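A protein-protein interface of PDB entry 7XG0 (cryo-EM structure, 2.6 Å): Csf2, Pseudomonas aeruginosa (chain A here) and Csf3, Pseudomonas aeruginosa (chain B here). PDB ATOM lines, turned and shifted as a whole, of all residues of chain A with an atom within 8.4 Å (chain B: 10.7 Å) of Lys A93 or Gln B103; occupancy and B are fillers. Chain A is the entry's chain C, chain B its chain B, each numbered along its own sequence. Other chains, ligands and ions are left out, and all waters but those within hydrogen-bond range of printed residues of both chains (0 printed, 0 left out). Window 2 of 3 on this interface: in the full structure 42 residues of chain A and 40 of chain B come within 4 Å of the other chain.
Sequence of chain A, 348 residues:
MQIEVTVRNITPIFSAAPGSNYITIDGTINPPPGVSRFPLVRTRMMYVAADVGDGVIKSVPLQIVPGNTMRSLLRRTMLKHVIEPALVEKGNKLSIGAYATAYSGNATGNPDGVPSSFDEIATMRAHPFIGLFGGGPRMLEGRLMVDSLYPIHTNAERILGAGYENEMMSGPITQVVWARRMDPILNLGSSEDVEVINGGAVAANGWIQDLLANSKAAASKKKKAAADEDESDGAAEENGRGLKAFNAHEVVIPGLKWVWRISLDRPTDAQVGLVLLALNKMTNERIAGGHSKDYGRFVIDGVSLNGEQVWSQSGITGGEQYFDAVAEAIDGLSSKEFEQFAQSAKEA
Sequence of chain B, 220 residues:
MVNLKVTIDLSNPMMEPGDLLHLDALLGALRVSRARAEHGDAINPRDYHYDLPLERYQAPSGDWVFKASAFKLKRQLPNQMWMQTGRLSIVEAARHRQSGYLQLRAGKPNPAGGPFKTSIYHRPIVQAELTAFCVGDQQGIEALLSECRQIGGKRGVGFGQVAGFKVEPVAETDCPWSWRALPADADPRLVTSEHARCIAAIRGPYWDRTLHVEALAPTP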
ATOM      1  N   ALA A  86      22.454  31.511  20.404  1.00  0.00           N
ATOM      2  CA  ALA A  86      23.283  30.553  21.132  1.00  0.00           C
ATOM      3  C   ALA A  86      22.841  29.119  20.866  1.00  0.00           C
ATOM      4  O   ALA A  86      23.676  28.209  20.767  1.00  0.00           O
ATOM      5  CB  ALA A  86      23.246  30.856  22.630  1.00  0.00           C
ATOM      6  N   LEU A  87      21.529  28.895  20.763  1.00  0.00           N
ATOM      7  CA  LEU A  87      21.039  27.553  20.469  1.00  0.00           C
ATOM      8  C   LEU A  87      21.237  27.201  19.001  1.00  0.00           C
ATOM      9  O   LEU A  87      21.401  26.026  18.652  1.00  0.00           O
ATOM     10  CB  LEU A  87      19.567  27.430  20.855  1.00  0.00           C
ATOM     11  CG  LEU A  87      19.218  27.494  22.344  1.00  0.00           C
ATOM     12  CD1 LEU A  87      17.779  27.062  22.558  1.00  0.00           C
ATOM     13  CD2 LEU A  87      20.164  26.644  23.173  1.00  0.00           C
ATOM     14  N   VAL A  88      21.197  28.205  18.122  1.00  0.00           N
ATOM     15  CA  VAL A  88      21.434  27.971  16.700  1.00  0.00           C
ATOM     16  C   VAL A  88      22.906  27.659  16.442  1.00  0.00           C
ATOM     17  O   VAL A  88      23.238  26.738  15.684  1.00  0.00           O
ATOM     18  CB  VAL A  88      20.934  29.178  15.879  1.00  0.00           C
ATOM     19  CG1 VAL A  88      21.708  29.357  14.573  1.00  0.00           C
ATOM     20  CG2 VAL A  88      19.454  29.017  15.573  1.00  0.00           C
ATOM     21  N   LYS A  90      25.237  26.307  18.204  1.00  0.00           N
ATOM     22  CA  LYS A  90      25.671  24.965  18.567  1.00  0.00           C
ATOM     23  C   LYS A  90      24.795  23.874  17.942  1.00  0.00           C
ATOM     24  O   LYS A  90      25.110  22.688  18.089  1.00  0.00           O
ATOM     25  CB  LYS A  90      25.717  24.806  20.092  1.00  0.00           C
ATOM     26  CG  LYS A  90      26.182  26.041  20.875  1.00  0.00           C
ATOM     27  CD  LYS A  90      26.652  25.652  22.282  1.00  0.00           C
ATOM     28  CE  LYS A  90      26.874  26.841  23.218  1.00  0.00           C
ATOM     29  NZ  LYS A  90      26.633  28.156  22.568  1.00  0.00           N
ATOM     30  N   GLY A  91      23.737  24.246  17.220  1.00  0.00           N
ATOM     31  CA  GLY A  91      22.911  23.281  16.515  1.00  0.00           C
ATOM     32  C   GLY A  91      21.832  22.654  17.368  1.00  0.00           C
ATOM     33  O   GLY A  91      21.228  21.646  16.982  1.00  0.00           O
ATOM     34  N   ASN A  92      21.590  23.239  18.536  1.00  0.00           N
ATOM     35  CA  ASN A  92      20.492  22.812  19.388  1.00  0.00           C
ATOM     36  C   ASN A  92      19.157  23.223  18.781  1.00  0.00           C
ATOM     37  O   ASN A  92      19.065  24.188  18.018  1.00  0.00           O
ATOM     38  CB  ASN A  92      20.624  23.400  20.792  1.00  0.00           C
ATOM     39  CG  ASN A  92      21.798  22.827  21.559  1.00  0.00           C
ATOM     40  OD1 ASN A  92      21.624  21.968  22.424  1.00  0.00           O
ATOM     41  ND2 ASN A  92      22.992  23.306  21.264  1.00  0.00           N
ATOM     42  N   LYS A  93      18.116  22.477  19.138  1.00  0.00           N
ATOM     43  CA  LYS A  93      16.818  22.594  18.500  1.00  0.00           C
ATOM     44  C   LYS A  93      15.731  22.461  19.558  1.00  0.00           C
ATOM     45  O   LYS A  93      15.916  21.773  20.564  1.00  0.00           O
ATOM     46  CB  LYS A  93      16.676  21.513  17.433  1.00  0.00           C
ATOM     47  CG  LYS A  93      17.146  21.963  16.067  1.00  0.00           C
ATOM     48  CD  LYS A  93      17.010  20.861  15.039  1.00  0.00           C
ATOM     49  CE  LYS A  93      17.583  21.277  13.689  1.00  0.00           C
ATOM     50  NZ  LYS A  93      18.782  22.158  13.819  1.00  0.00           N
ATOM     51  N   LEU A  94      14.595  23.114  19.328  1.00  0.00           N
ATOM     52  CA  LEU A  94      13.507  23.135  20.298  1.00  0.00           C
ATOM     53  C   LEU A  94      12.277  22.429  19.749  1.00  0.00           C
ATOM     54  O   LEU A  94      11.885  22.652  18.598  1.00  0.00           O
ATOM     55  CB  LEU A  94      13.134  24.567  20.697  1.00  0.00           C
ATOM     56  CG  LEU A  94      14.139  25.379  21.513  1.00  0.00           C
ATOM     57  CD1 LEU A  94      13.544  26.728  21.859  1.00  0.00           C
ATOM     58  CD2 LEU A  94      14.530  24.635  22.776  1.00  0.00           C
ATOM     59  N   SER A  95      11.672  21.584  20.579  1.00  0.00           N
ATOM     60  CA  SER A  95      10.341  21.073  20.310  1.00  0.00           C
ATOM     61  C   SER A  95       9.302  22.153  20.609  1.00  0.00           C
ATOM     62  O   SER A  95       9.614  23.212  21.161  1.00  0.00           O
ATOM     63  CB  SER A  95      10.071  19.818  21.140  1.00  0.00           C
ATOM     64  OG  SER A  95       9.994  20.132  22.519  1.00  0.00           O
ATOM     65  N   ILE A  96       8.050  21.872  20.232  1.00  0.00           N
ATOM     66  CA  ILE A  96       6.982  22.862  20.368  1.00  0.00           C
ATOM     67  C   ILE A  96       6.663  23.141  21.838  1.00  0.00           C
ATOM     68  O   ILE A  96       6.344  24.282  22.202  1.00  0.00           O
ATOM     69  CB  ILE A  96       5.742  22.413  19.559  1.00  0.00           C
ATOM     70  CG1 ILE A  96       4.654  23.493  19.562  1.00  0.00           C
ATOM     71  CG2 ILE A  96       5.208  21.050  20.013  1.00  0.00           C
ATOM     72  CD1 ILE A  96       5.128  24.840  19.067  1.00  0.00           C
ATOM     73  N   GLY A  97       6.783  22.133  22.705  1.00  0.00           N
ATOM     74  CA  GLY A  97       6.601  22.367  24.129  1.00  0.00           C
ATOM     75  C   GLY A  97       7.693  23.238  24.718  1.00  0.00           C
ATOM     76  O   GLY A  97       7.415  24.179  25.469  1.00  0.00           O
ATOM     77  N   ALA A  98       8.950  22.956  24.357  1.00  0.00           N
ATOM     78  CA  ALA A  98      10.067  23.756  24.848  1.00  0.00           C
ATOM     79  C   ALA A  98      10.046  25.160  24.259  1.00  0.00           C
ATOM     80  O   ALA A  98      10.369  26.133  24.953  1.00  0.00           O
ATOM     81  CB  ALA A  98      11.390  23.061  24.529  1.00  0.00           C
ATOM     82  N   TYR A  99       9.648  25.286  22.989  1.00  0.00           N
ATOM     83  CA  TYR A  99       9.542  26.596  22.352  1.00  0.00           C
ATOM     84  C   TYR A  99       8.447  27.437  22.998  1.00  0.00           C
ATOM     85  O   TYR A  99       8.646  28.626  23.270  1.00  0.00           O
ATOM     86  CB  TYR A  99       9.277  26.435  20.854  1.00  0.00           C
ATOM     87  CG  TYR A  99       9.237  27.738  20.093  1.00  0.00           C
ATOM     88  CD1 TYR A  99      10.409  28.379  19.723  1.00  0.00           C
ATOM     89  CD2 TYR A  99       8.025  28.321  19.732  1.00  0.00           C
ATOM     90  CE1 TYR A  99      10.380  29.567  19.027  1.00  0.00           C
ATOM     91  CE2 TYR A  99       7.986  29.514  19.035  1.00  0.00           C
ATOM     92  CZ  TYR A  99       9.168  30.130  18.685  1.00  0.00           C
ATOM     93  OH  TYR A  99       9.144  31.317  17.990  1.00  0.00           O
ATOM     94  N   SER A 334      22.469  24.953  26.354  1.00  0.00           N
ATOM     95  CA  SER A 334      21.941  23.975  25.419  1.00  0.00           C
ATOM     96  C   SER A 334      20.425  23.907  25.548  1.00  0.00           C
ATOM     97  O   SER A 334      19.838  24.404  26.514  1.00  0.00           O
ATOM     98  CB  SER A 334      22.550  22.588  25.659  1.00  0.00           C
ATOM     99  OG  SER A 334      22.237  22.111  26.956  1.00  0.00           O
ATOM    100  N   SER A 335      19.792  23.282  24.555  1.00  0.00           N
ATOM    101  CA  SER A 335      18.343  23.124  24.578  1.00  0.00           C
ATOM    102  C   SER A 335      17.887  21.971  25.459  1.00  0.00           C
ATOM    103  O   SER A 335      16.678  21.820  25.655  1.00  0.00           O
ATOM    104  CB  SER A 335      17.808  22.919  23.162  1.00  0.00           C
ATOM    105  OG  SER A 335      18.207  21.664  22.642  1.00  0.00           O
ATOM    106  N   LYS A 336      18.818  21.157  25.971  1.00  0.00           N
ATOM    107  CA  LYS A 336      18.455  20.034  26.832  1.00  0.00           C
ATOM    108  C   LYS A 336      17.821  20.514  28.131  1.00  0.00           C
ATOM    109  O   LYS A 336      16.856  19.912  28.621  1.00  0.00           O
ATOM    110  CB  LYS A 336      19.692  19.181  27.120  1.00  0.00           C
ATOM    111  CG  LYS A 336      19.423  17.935  27.948  1.00  0.00           C
ATOM    112  CD  LYS A 336      20.719  17.296  28.417  1.00  0.00           C
ATOM    113  CE  LYS A 336      20.562  16.683  29.799  1.00  0.00           C
ATOM    114  NZ  LYS A 336      20.819  17.678  30.877  1.00  0.00           N
ATOM    115  N   PHE A 338      16.134  23.314  28.390  1.00  0.00           N
ATOM    116  CA  PHE A 338      14.811  23.807  28.006  1.00  0.00           C
ATOM    117  C   PHE A 338      13.814  22.664  27.837  1.00  0.00           C
ATOM    118  O   PHE A 338      12.665  22.759  28.290  1.00  0.00           O
ATOM    119  CB  PHE A 338      14.910  24.612  26.709  1.00  0.00           C
ATOM    120  CG  PHE A 338      15.548  25.963  26.875  1.00  0.00           C
ATOM    121  CD1 PHE A 338      16.928  26.104  26.854  1.00  0.00           C
ATOM    122  CD2 PHE A 338      14.765  27.094  27.042  1.00  0.00           C
ATOM    123  CE1 PHE A 338      17.515  27.349  27.003  1.00  0.00           C
ATOM    124  CE2 PHE A 338      15.344  28.340  27.192  1.00  0.00           C
ATOM    125  CZ  PHE A 338      16.721  28.468  27.173  1.00  0.00           C
ATOM    126  N   GLU A 339      14.240  21.571  27.197  1.00  0.00           N
ATOM    127  CA  GLU A 339      13.346  20.438  26.969  1.00  0.00           C
ATOM    128  C   GLU A 339      13.038  19.703  28.269  1.00  0.00           C
ATOM    129  O   GLU A 339      11.926  19.194  28.448  1.00  0.00           O
ATOM    130  CB  GLU A 339      13.950  19.478  25.941  1.00  0.00           C
ATOM    131  CG  GLU A 339      14.176  20.078  24.558  1.00  0.00           C
ATOM    132  CD  GLU A 339      12.976  19.949  23.643  1.00  0.00           C
ATOM    133  OE1 GLU A 339      11.952  19.385  24.075  1.00  0.00           O
ATOM    134  OE2 GLU A 339      13.061  20.415  22.488  1.00  0.00           O
ATOM    135  N   GLU B  92       7.431  34.898  14.663  1.00  0.00           N
ATOM    136  CA  GLU B  92       8.684  34.322  15.133  1.00  0.00           C
ATOM    137  C   GLU B  92       8.623  32.801  15.120  1.00  0.00           C
ATOM    138  O   GLU B  92       9.630  32.138  14.856  1.00  0.00           O
ATOM    139  CB  GLU B  92       9.011  34.839  16.533  1.00  0.00           C
ATOM    140  CG  GLU B  92       9.352  36.327  16.609  1.00  0.00           C
ATOM    141  CD  GLU B  92      10.386  36.762  15.589  1.00  0.00           C
ATOM    142  OE1 GLU B  92      11.594  36.626  15.876  1.00  0.00           O
ATOM    143  OE2 GLU B  92       9.998  37.271  14.515  1.00  0.00           O
ATOM    144  N   ALA B  93       7.435  32.240  15.370  1.00  0.00           N
ATOM    145  CA  ALA B  93       7.252  30.794  15.283  1.00  0.00           C
ATOM    146  C   ALA B  93       7.454  30.288  13.861  1.00  0.00           C
ATOM    147  O   ALA B  93       8.098  29.256  13.652  1.00  0.00           O
ATOM    148  CB  ALA B  93       5.866  30.410  15.790  1.00  0.00           C
ATOM    149  N   ALA B  94       6.936  31.017  12.868  1.00  0.00           N
ATOM    150  CA  ALA B  94       7.113  30.605  11.476  1.00  0.00           C
ATOM    151  C   ALA B  94       8.566  30.746  11.032  1.00  0.00           C
ATOM    152  O   ALA B  94       9.082  29.905  10.281  1.00  0.00           O
ATOM    153  CB  ALA B  94       6.193  31.417  10.568  1.00  0.00           C
ATOM    154  N   ARG B  95       9.239  31.810  11.487  1.00  0.00           N
ATOM    155  CA  ARG B  95      10.652  31.992  11.155  1.00  0.00           C
ATOM    156  C   ARG B  95      11.516  30.898  11.777  1.00  0.00           C
ATOM    157  O   ARG B  95      12.413  30.352  11.118  1.00  0.00           O
ATOM    158  CB  ARG B  95      11.126  33.373  11.608  1.00  0.00           C
ATOM    159  CG  ARG B  95      12.537  33.717  11.158  1.00  0.00           C
ATOM    160  CD  ARG B  95      12.958  35.100  11.633  1.00  0.00           C
ATOM    161  NE  ARG B  95      13.089  35.171  13.084  1.00  0.00           N
ATOM    162  CZ  ARG B  95      14.181  34.832  13.753  1.00  0.00           C
ATOM    163  NH1 ARG B  95      15.261  34.385  13.134  1.00  0.00           N
ATOM    164  NH2 ARG B  95      14.191  34.946  15.078  1.00  0.00           N
ATOM    165  N   HIS B  96      11.238  30.538  13.034  1.00  0.00           N
ATOM    166  CA  HIS B  96      11.977  29.461  13.685  1.00  0.00           C
ATOM    167  C   HIS B  96      11.616  28.103  13.092  1.00  0.00           C
ATOM    168  O   HIS B  96      12.414  27.162  13.154  1.00  0.00           O
ATOM    169  CB  HIS B  96      11.708  29.479  15.189  1.00  0.00           C
ATOM    170  CG  HIS B  96      12.151  30.738  15.865  1.00  0.00           C
ATOM    171  ND1 HIS B  96      11.290  31.525  16.602  1.00  0.00           N
ATOM    172  CD2 HIS B  96      13.357  31.350  15.917  1.00  0.00           C
ATOM    173  CE1 HIS B  96      11.947  32.564  17.079  1.00  0.00           C
ATOM    174  NE2 HIS B  96      13.203  32.483  16.679  1.00  0.00           N
ATOM    175  N   ARG B  97      10.413  27.980  12.524  1.00  0.00           N
ATOM    176  CA  ARG B  97      10.004  26.708  11.943  1.00  0.00           C
ATOM    177  C   ARG B  97      10.652  26.489  10.579  1.00  0.00           C
ATOM    178  O   ARG B  97      10.999  25.353  10.230  1.00  0.00           O
ATOM    179  CB  ARG B  97       8.478  26.645  11.860  1.00  0.00           C
ATOM    180  CG  ARG B  97       7.916  25.289  11.461  1.00  0.00           C
ATOM    181  CD  ARG B  97       6.489  25.413  10.962  1.00  0.00           C
ATOM    182  NE  ARG B  97       5.937  24.139  10.520  1.00  0.00           N
ATOM    183  CZ  ARG B  97       5.371  23.940   9.338  1.00  0.00           C
ATOM    184  NH1 ARG B  97       5.259  24.917   8.453  1.00  0.00           N
ATOM    185  NH2 ARG B  97       4.902  22.733   9.038  1.00  0.00           N
ATOM    186  N   GLN B  98      10.824  27.558   9.788  1.00  0.00           N
ATOM    187  CA  GLN B  98      11.643  27.413   8.583  1.00  0.00           C
ATOM    188  C   GLN B  98      13.115  27.217   8.924  1.00  0.00           C
ATOM    189  O   GLN B  98      13.799  26.415   8.278  1.00  0.00           O
ATOM    190  CB  GLN B  98      11.508  28.601   7.628  1.00  0.00           C
ATOM    191  CG  GLN B  98      11.281  28.140   6.183  1.00  0.00           C
ATOM    192  CD  GLN B  98      10.540  29.137   5.321  1.00  0.00           C
ATOM    193  OE1 GLN B  98      10.765  30.341   5.421  1.00  0.00           O
ATOM    194  NE2 GLN B  98       9.660  28.640   4.459  1.00  0.00           N
ATOM    195  N   SER B  99      13.626  27.936   9.929  1.00  0.00           N
ATOM    196  CA  SER B  99      15.049  27.833  10.238  1.00  0.00           C
ATOM    197  C   SER B  99      15.421  26.523  10.922  1.00  0.00           C
ATOM    198  O   SER B  99      16.614  26.220  11.029  1.00  0.00           O
ATOM    199  CB  SER B  99      15.493  29.010  11.110  1.00  0.00           C
ATOM    200  OG  SER B  99      14.979  28.894  12.422  1.00  0.00           O
ATOM    201  N   GLY B 100      14.441  25.738  11.374  1.00  0.00           N
ATOM    202  CA  GLY B 100      14.689  24.463  12.004  1.00  0.00           C
ATOM    203  C   GLY B 100      14.881  24.519  13.502  1.00  0.00           C
ATOM    204  O   GLY B 100      14.935  23.463  14.143  1.00  0.00           O
ATOM    205  N   TYR B 101      14.976  25.721  14.077  1.00  0.00           N
ATOM    206  CA  TYR B 101      15.202  25.859  15.513  1.00  0.00           C
ATOM    207  C   TYR B 101      13.964  25.453  16.305  1.00  0.00           C
ATOM    208  O   TYR B 101      14.077  25.031  17.462  1.00  0.00           O
ATOM    209  CB  TYR B 101      15.668  27.300  15.801  1.00  0.00           C
ATOM    210  CG  TYR B 101      15.509  27.862  17.208  1.00  0.00           C
ATOM    211  CD1 TYR B 101      14.304  28.422  17.648  1.00  0.00           C
ATOM    212  CD2 TYR B 101      16.616  27.982  18.038  1.00  0.00           C
ATOM    213  CE1 TYR B 101      14.188  28.963  18.914  1.00  0.00           C
ATOM    214  CE2 TYR B 101      16.508  28.522  19.303  1.00  0.00           C
ATOM    215  CZ  TYR B 101      15.295  29.018  19.733  1.00  0.00           C
ATOM    216  OH  TYR B 101      15.194  29.566  20.990  1.00  0.00           O
ATOM    217  N   LEU B 102      12.785  25.582  15.706  1.00  0.00           N
ATOM    218  CA  LEU B 102      11.543  25.061  16.260  1.00  0.00           C
ATOM    219  C   LEU B 102      11.140  23.846  15.435  1.00  0.00           C
ATOM    220  O   LEU B 102      10.839  23.972  14.243  1.00  0.00           O
ATOM    221  CB  LEU B 102      10.447  26.129  16.246  1.00  0.00           C
ATOM    222  CG  LEU B 102       8.955  25.756  16.264  1.00  0.00           C
ATOM    223  CD1 LEU B 102       8.557  24.980  17.514  1.00  0.00           C
ATOM    224  CD2 LEU B 102       8.078  26.987  16.090  1.00  0.00           C
ATOM    225  N   GLN B 103      11.153  22.671  16.064  1.00  0.00           N
ATOM    226  CA  GLN B 103      10.640  21.456  15.435  1.00  0.00           C
ATOM    227  C   GLN B 103       9.139  21.347  15.693  1.00  0.00           C
ATOM    228  O   GLN B 103       8.666  20.701  16.629  1.00  0.00           O
ATOM    229  CB  GLN B 103      11.401  20.232  15.925  1.00  0.00           C
ATOM    230  CG  GLN B 103      12.890  20.322  15.673  1.00  0.00           C
ATOM    231  CD  GLN B 103      13.231  20.014  14.229  1.00  0.00           C
ATOM    232  OE1 GLN B 103      14.099  20.649  13.630  1.00  0.00           O
ATOM    233  NE2 GLN B 103      12.558  19.019  13.662  1.00  0.00           N
ATOM    234  N   LEU B 104       8.392  22.030  14.836  1.00  0.00           N
ATOM    235  CA  LEU B 104       6.941  21.947  14.801  1.00  0.00           C
ATOM    236  C   LEU B 104       6.533  21.339  13.469  1.00  0.00           C
ATOM    237  O   LEU B 104       6.846  21.891  12.409  1.00  0.00           O
ATOM    238  CB  LEU B 104       6.304  23.322  14.977  1.00  0.00           C
ATOM    239  CG  LEU B 104       4.778  23.338  14.959  1.00  0.00           C
ATOM    240  CD1 LEU B 104       4.204  22.447  16.042  1.00  0.00           C
ATOM    241  CD2 LEU B 104       4.287  24.750  15.112  1.00  0.00           C
ATOM    242  N   ARG B 105       5.846  20.204  13.525  1.00  0.00           N
ATOM    243  CA  ARG B 105       5.348  19.568  12.316  1.00  0.00           C
ATOM    244  C   ARG B 105       4.036  20.190  11.856  1.00  0.00           C
ATOM    245  O   ARG B 105       3.678  20.077  10.676  1.00  0.00           O
ATOM    246  CB  ARG B 105       5.189  18.063  12.563  1.00  0.00           C
ATOM    247  CG  ARG B 105       4.980  17.205  11.323  1.00  0.00           C
ATOM    248  CD  ARG B 105       5.959  16.020  11.283  1.00  0.00           C
ATOM    249  NE  ARG B 105       6.093  15.263  12.530  1.00  0.00           N
ATOM    250  CZ  ARG B 105       5.130  14.599  13.164  1.00  0.00           C
ATOM    251  NH1 ARG B 105       3.928  14.429  12.635  1.00  0.00           N
ATOM    252  NH2 ARG B 105       5.394  14.055  14.348  1.00  0.00           N
ATOM    253  N   ALA B 106       3.334  20.872  12.758  1.00  0.00           N
ATOM    254  CA  ALA B 106       2.051  21.479  12.432  1.00  0.00           C
ATOM    255  C   ALA B 106       2.220  22.671  11.498  1.00  0.00           C
ATOM    256  O   ALA B 106       3.088  23.528  11.691  1.00  0.00           O
ATOM    257  CB  ALA B 106       1.331  21.919  13.706  1.00  0.00           C
ATOM    258  N   GLY B 107       1.369  22.719  10.478  1.00  0.00           N
ATOM    259  CA  GLY B 107       1.403  23.798   9.515  1.00  0.00           C
ATOM    260  C   GLY B 107       0.601  25.006   9.951  1.00  0.00           C
ATOM    261  O   GLY B 107       1.043  26.140   9.767  1.00  0.00           O
ATOM    262  N   PRO B 115      -0.435  25.711  21.720  1.00  0.00           N
ATOM    263  CA  PRO B 115       0.700  26.595  22.037  1.00  0.00           C
ATOM    264  C   PRO B 115       0.517  28.016  21.548  1.00  0.00           C
ATOM    265  O   PRO B 115       1.080  28.947  22.138  1.00  0.00           O
ATOM    266  CB  PRO B 115       1.889  25.908  21.345  1.00  0.00           C
ATOM    267  CG  PRO B 115       1.400  24.535  20.966  1.00  0.00           C
ATOM    268  CD  PRO B 115      -0.065  24.658  20.762  1.00  0.00           C
ATOM    269  N   PHE B 116      -0.269  28.212  20.495  1.00  0.00           N
ATOM    270  CA  PHE B 116      -0.482  29.520  19.895  1.00  0.00           C
ATOM    271  C   PHE B 116      -1.848  30.088  20.257  1.00  0.00           C
ATOM    272  O   PHE B 116      -2.383  30.941  19.546  1.00  0.00           O
ATOM    273  CB  PHE B 116      -0.311  29.429  18.382  1.00  0.00           C
ATOM    274  CG  PHE B 116       0.946  28.731  17.975  1.00  0.00           C
ATOM    275  CD1 PHE B 116       2.161  29.388  18.043  1.00  0.00           C
ATOM    276  CD2 PHE B 116       0.920  27.411  17.552  1.00  0.00           C
ATOM    277  CE1 PHE B 116       3.326  28.750  17.686  1.00  0.00           C
ATOM    278  CE2 PHE B 116       2.085  26.767  17.192  1.00  0.00           C
ATOM    279  CZ  PHE B 116       3.291  27.441  17.263  1.00  0.00           C
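Of the 18 printed residues of chain A, 6 touch a printed residue of chain B. Printed residues of chain B that touch a printed residue of chain A: Glu B92, Ala B93, His B96, Gly B100, Tyr B101, Leu B102, Gln B103, Leu B104, Pro B115 and Phe B116. Hydrophobic or aromatic side chains of chain B that line the printed part of chain A: Ala B93, His B96, Tyr B101, Leu B102, Leu B104, Pro B115 and Phe B116. Among the printed residues, 18 pairs touch across the chains. Among the printed residues, no Asp or Glu carboxylate lies within 4 Å of a Lys or Arg side-chain nitrogen of the other chain.
The side-chain hydroxyl (OH) of Tyr A99 sits close to the backbone carbonyl oxygen (O) of Glu B92 (3.3 Å). The side-chain hydroxyl (OH) of Tyr A99 lies within hydrogen-bond range of the backbone NH (N) of Ala B93, at 3.3 Å. ND1 of His B96 lies within hydrogen-bond range of OH of Tyr A99. The backbone NH of Leu A94 lies within hydrogen-bond range of the backbone carbonyl oxygen of Tyr B101 (2.7 Å). N of Gln B103 sits at hydrogen-bond distance from O of Leu A94 (2.6 Å).
Among the printed residues, pairs that only touch across the chains: Leu A87 with Tyr B101 (3.6 Å), Val A88 with Tyr B101 (3.9 Å), Lys A93 with Gly B100 (3.3 Å), Lys A93 with Tyr B101 (3.7 Å), Lys A93 with Gln B103 (3.2 Å), Leu A94 with Leu B102 (3.4 Å), Ile A96 with Leu B102 (3.8 Å), Ile A96 with Gln B103 (3.8 Å), Ile A96 with Leu B104 (3.7 Å), Ile A96 with Pro B115 (3.7 Å), Ile A96 with Phe B116 (3.7 Å), Tyr A99 with Tyr B101 (3.9 Å) and Tyr A99 with Leu B102 (3.7 Å).
The guanidinium group (NH2) of Arg B95 lies within salt-bridge range of the side-chain carboxylate (OE1) of Glu B92 (3.2 Å). N of Tyr B101 sits at hydrogen-bond distance from O of His B96 (3.1 Å). O of His B96 lies within hydrogen-bond range of N of Leu B102 (3.0 Å). O of Leu B104 is in hydrogen-bond range of NE of Arg B97. The side-chain amide oxygen (OE1) of Gln B103 lies close to the backbone carbonyl oxygen (O) of Gly B100 (3.0 Å). The backbone NH (N) of Asn A92 sits at hydrogen-bond distance from the backbone carbonyl oxygen (O) of Leu A87 (2.8 Å).
Of chain B, only Gly B100 (3.3 Å), Tyr B101 (3.7 Å) and Gln B103 (3.2 Å) come within 4 Å of Lys A93. Printed residues of chain A within 4 Å of Gln B103: Lys A93 (3.2 Å), Leu A94 (2.6 Å) and Ile A96 (3.8 Å). No residue of chain B comes within 4 Å of Gly A91. No residue of chain B comes within 4 Å of Asn A92. Of chain B, only Tyr B101 (2.7 Å), Leu B102 (3.4 Å) and Gln B103 (2.6 Å) come within 4 Å of Leu A94. No residue of chain B comes within 4 Å of Ser A95. No residue of chain B comes within 4 Å of Ser A335. Printed residues of chain B within 4 Å of Ile A96: Leu B102, Gln B103, Leu B104, Pro B115 and Phe B116. Of the printed residues of chain B, Val A88 touches Tyr B101 (3.9 Å). Of the printed residues of chain A, Pro B115 touches Ile A96. Of the printed residues of chain B, Tyr A99 touches Glu B92 (3.3 Å), Ala B93 (3.3 Å), His B96 (2.6 Å), Tyr B101 (3.9 Å) and Leu B102 (3.7 Å). Ala B94 touches none of the printed residues of chain A. The nearest residue of chain A that does not touch Gln B103 is Ser A95 (4.1 Å). The nearest printed residue of chain B that does not touch Val A88 is Ser B99 (5.5 Å).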
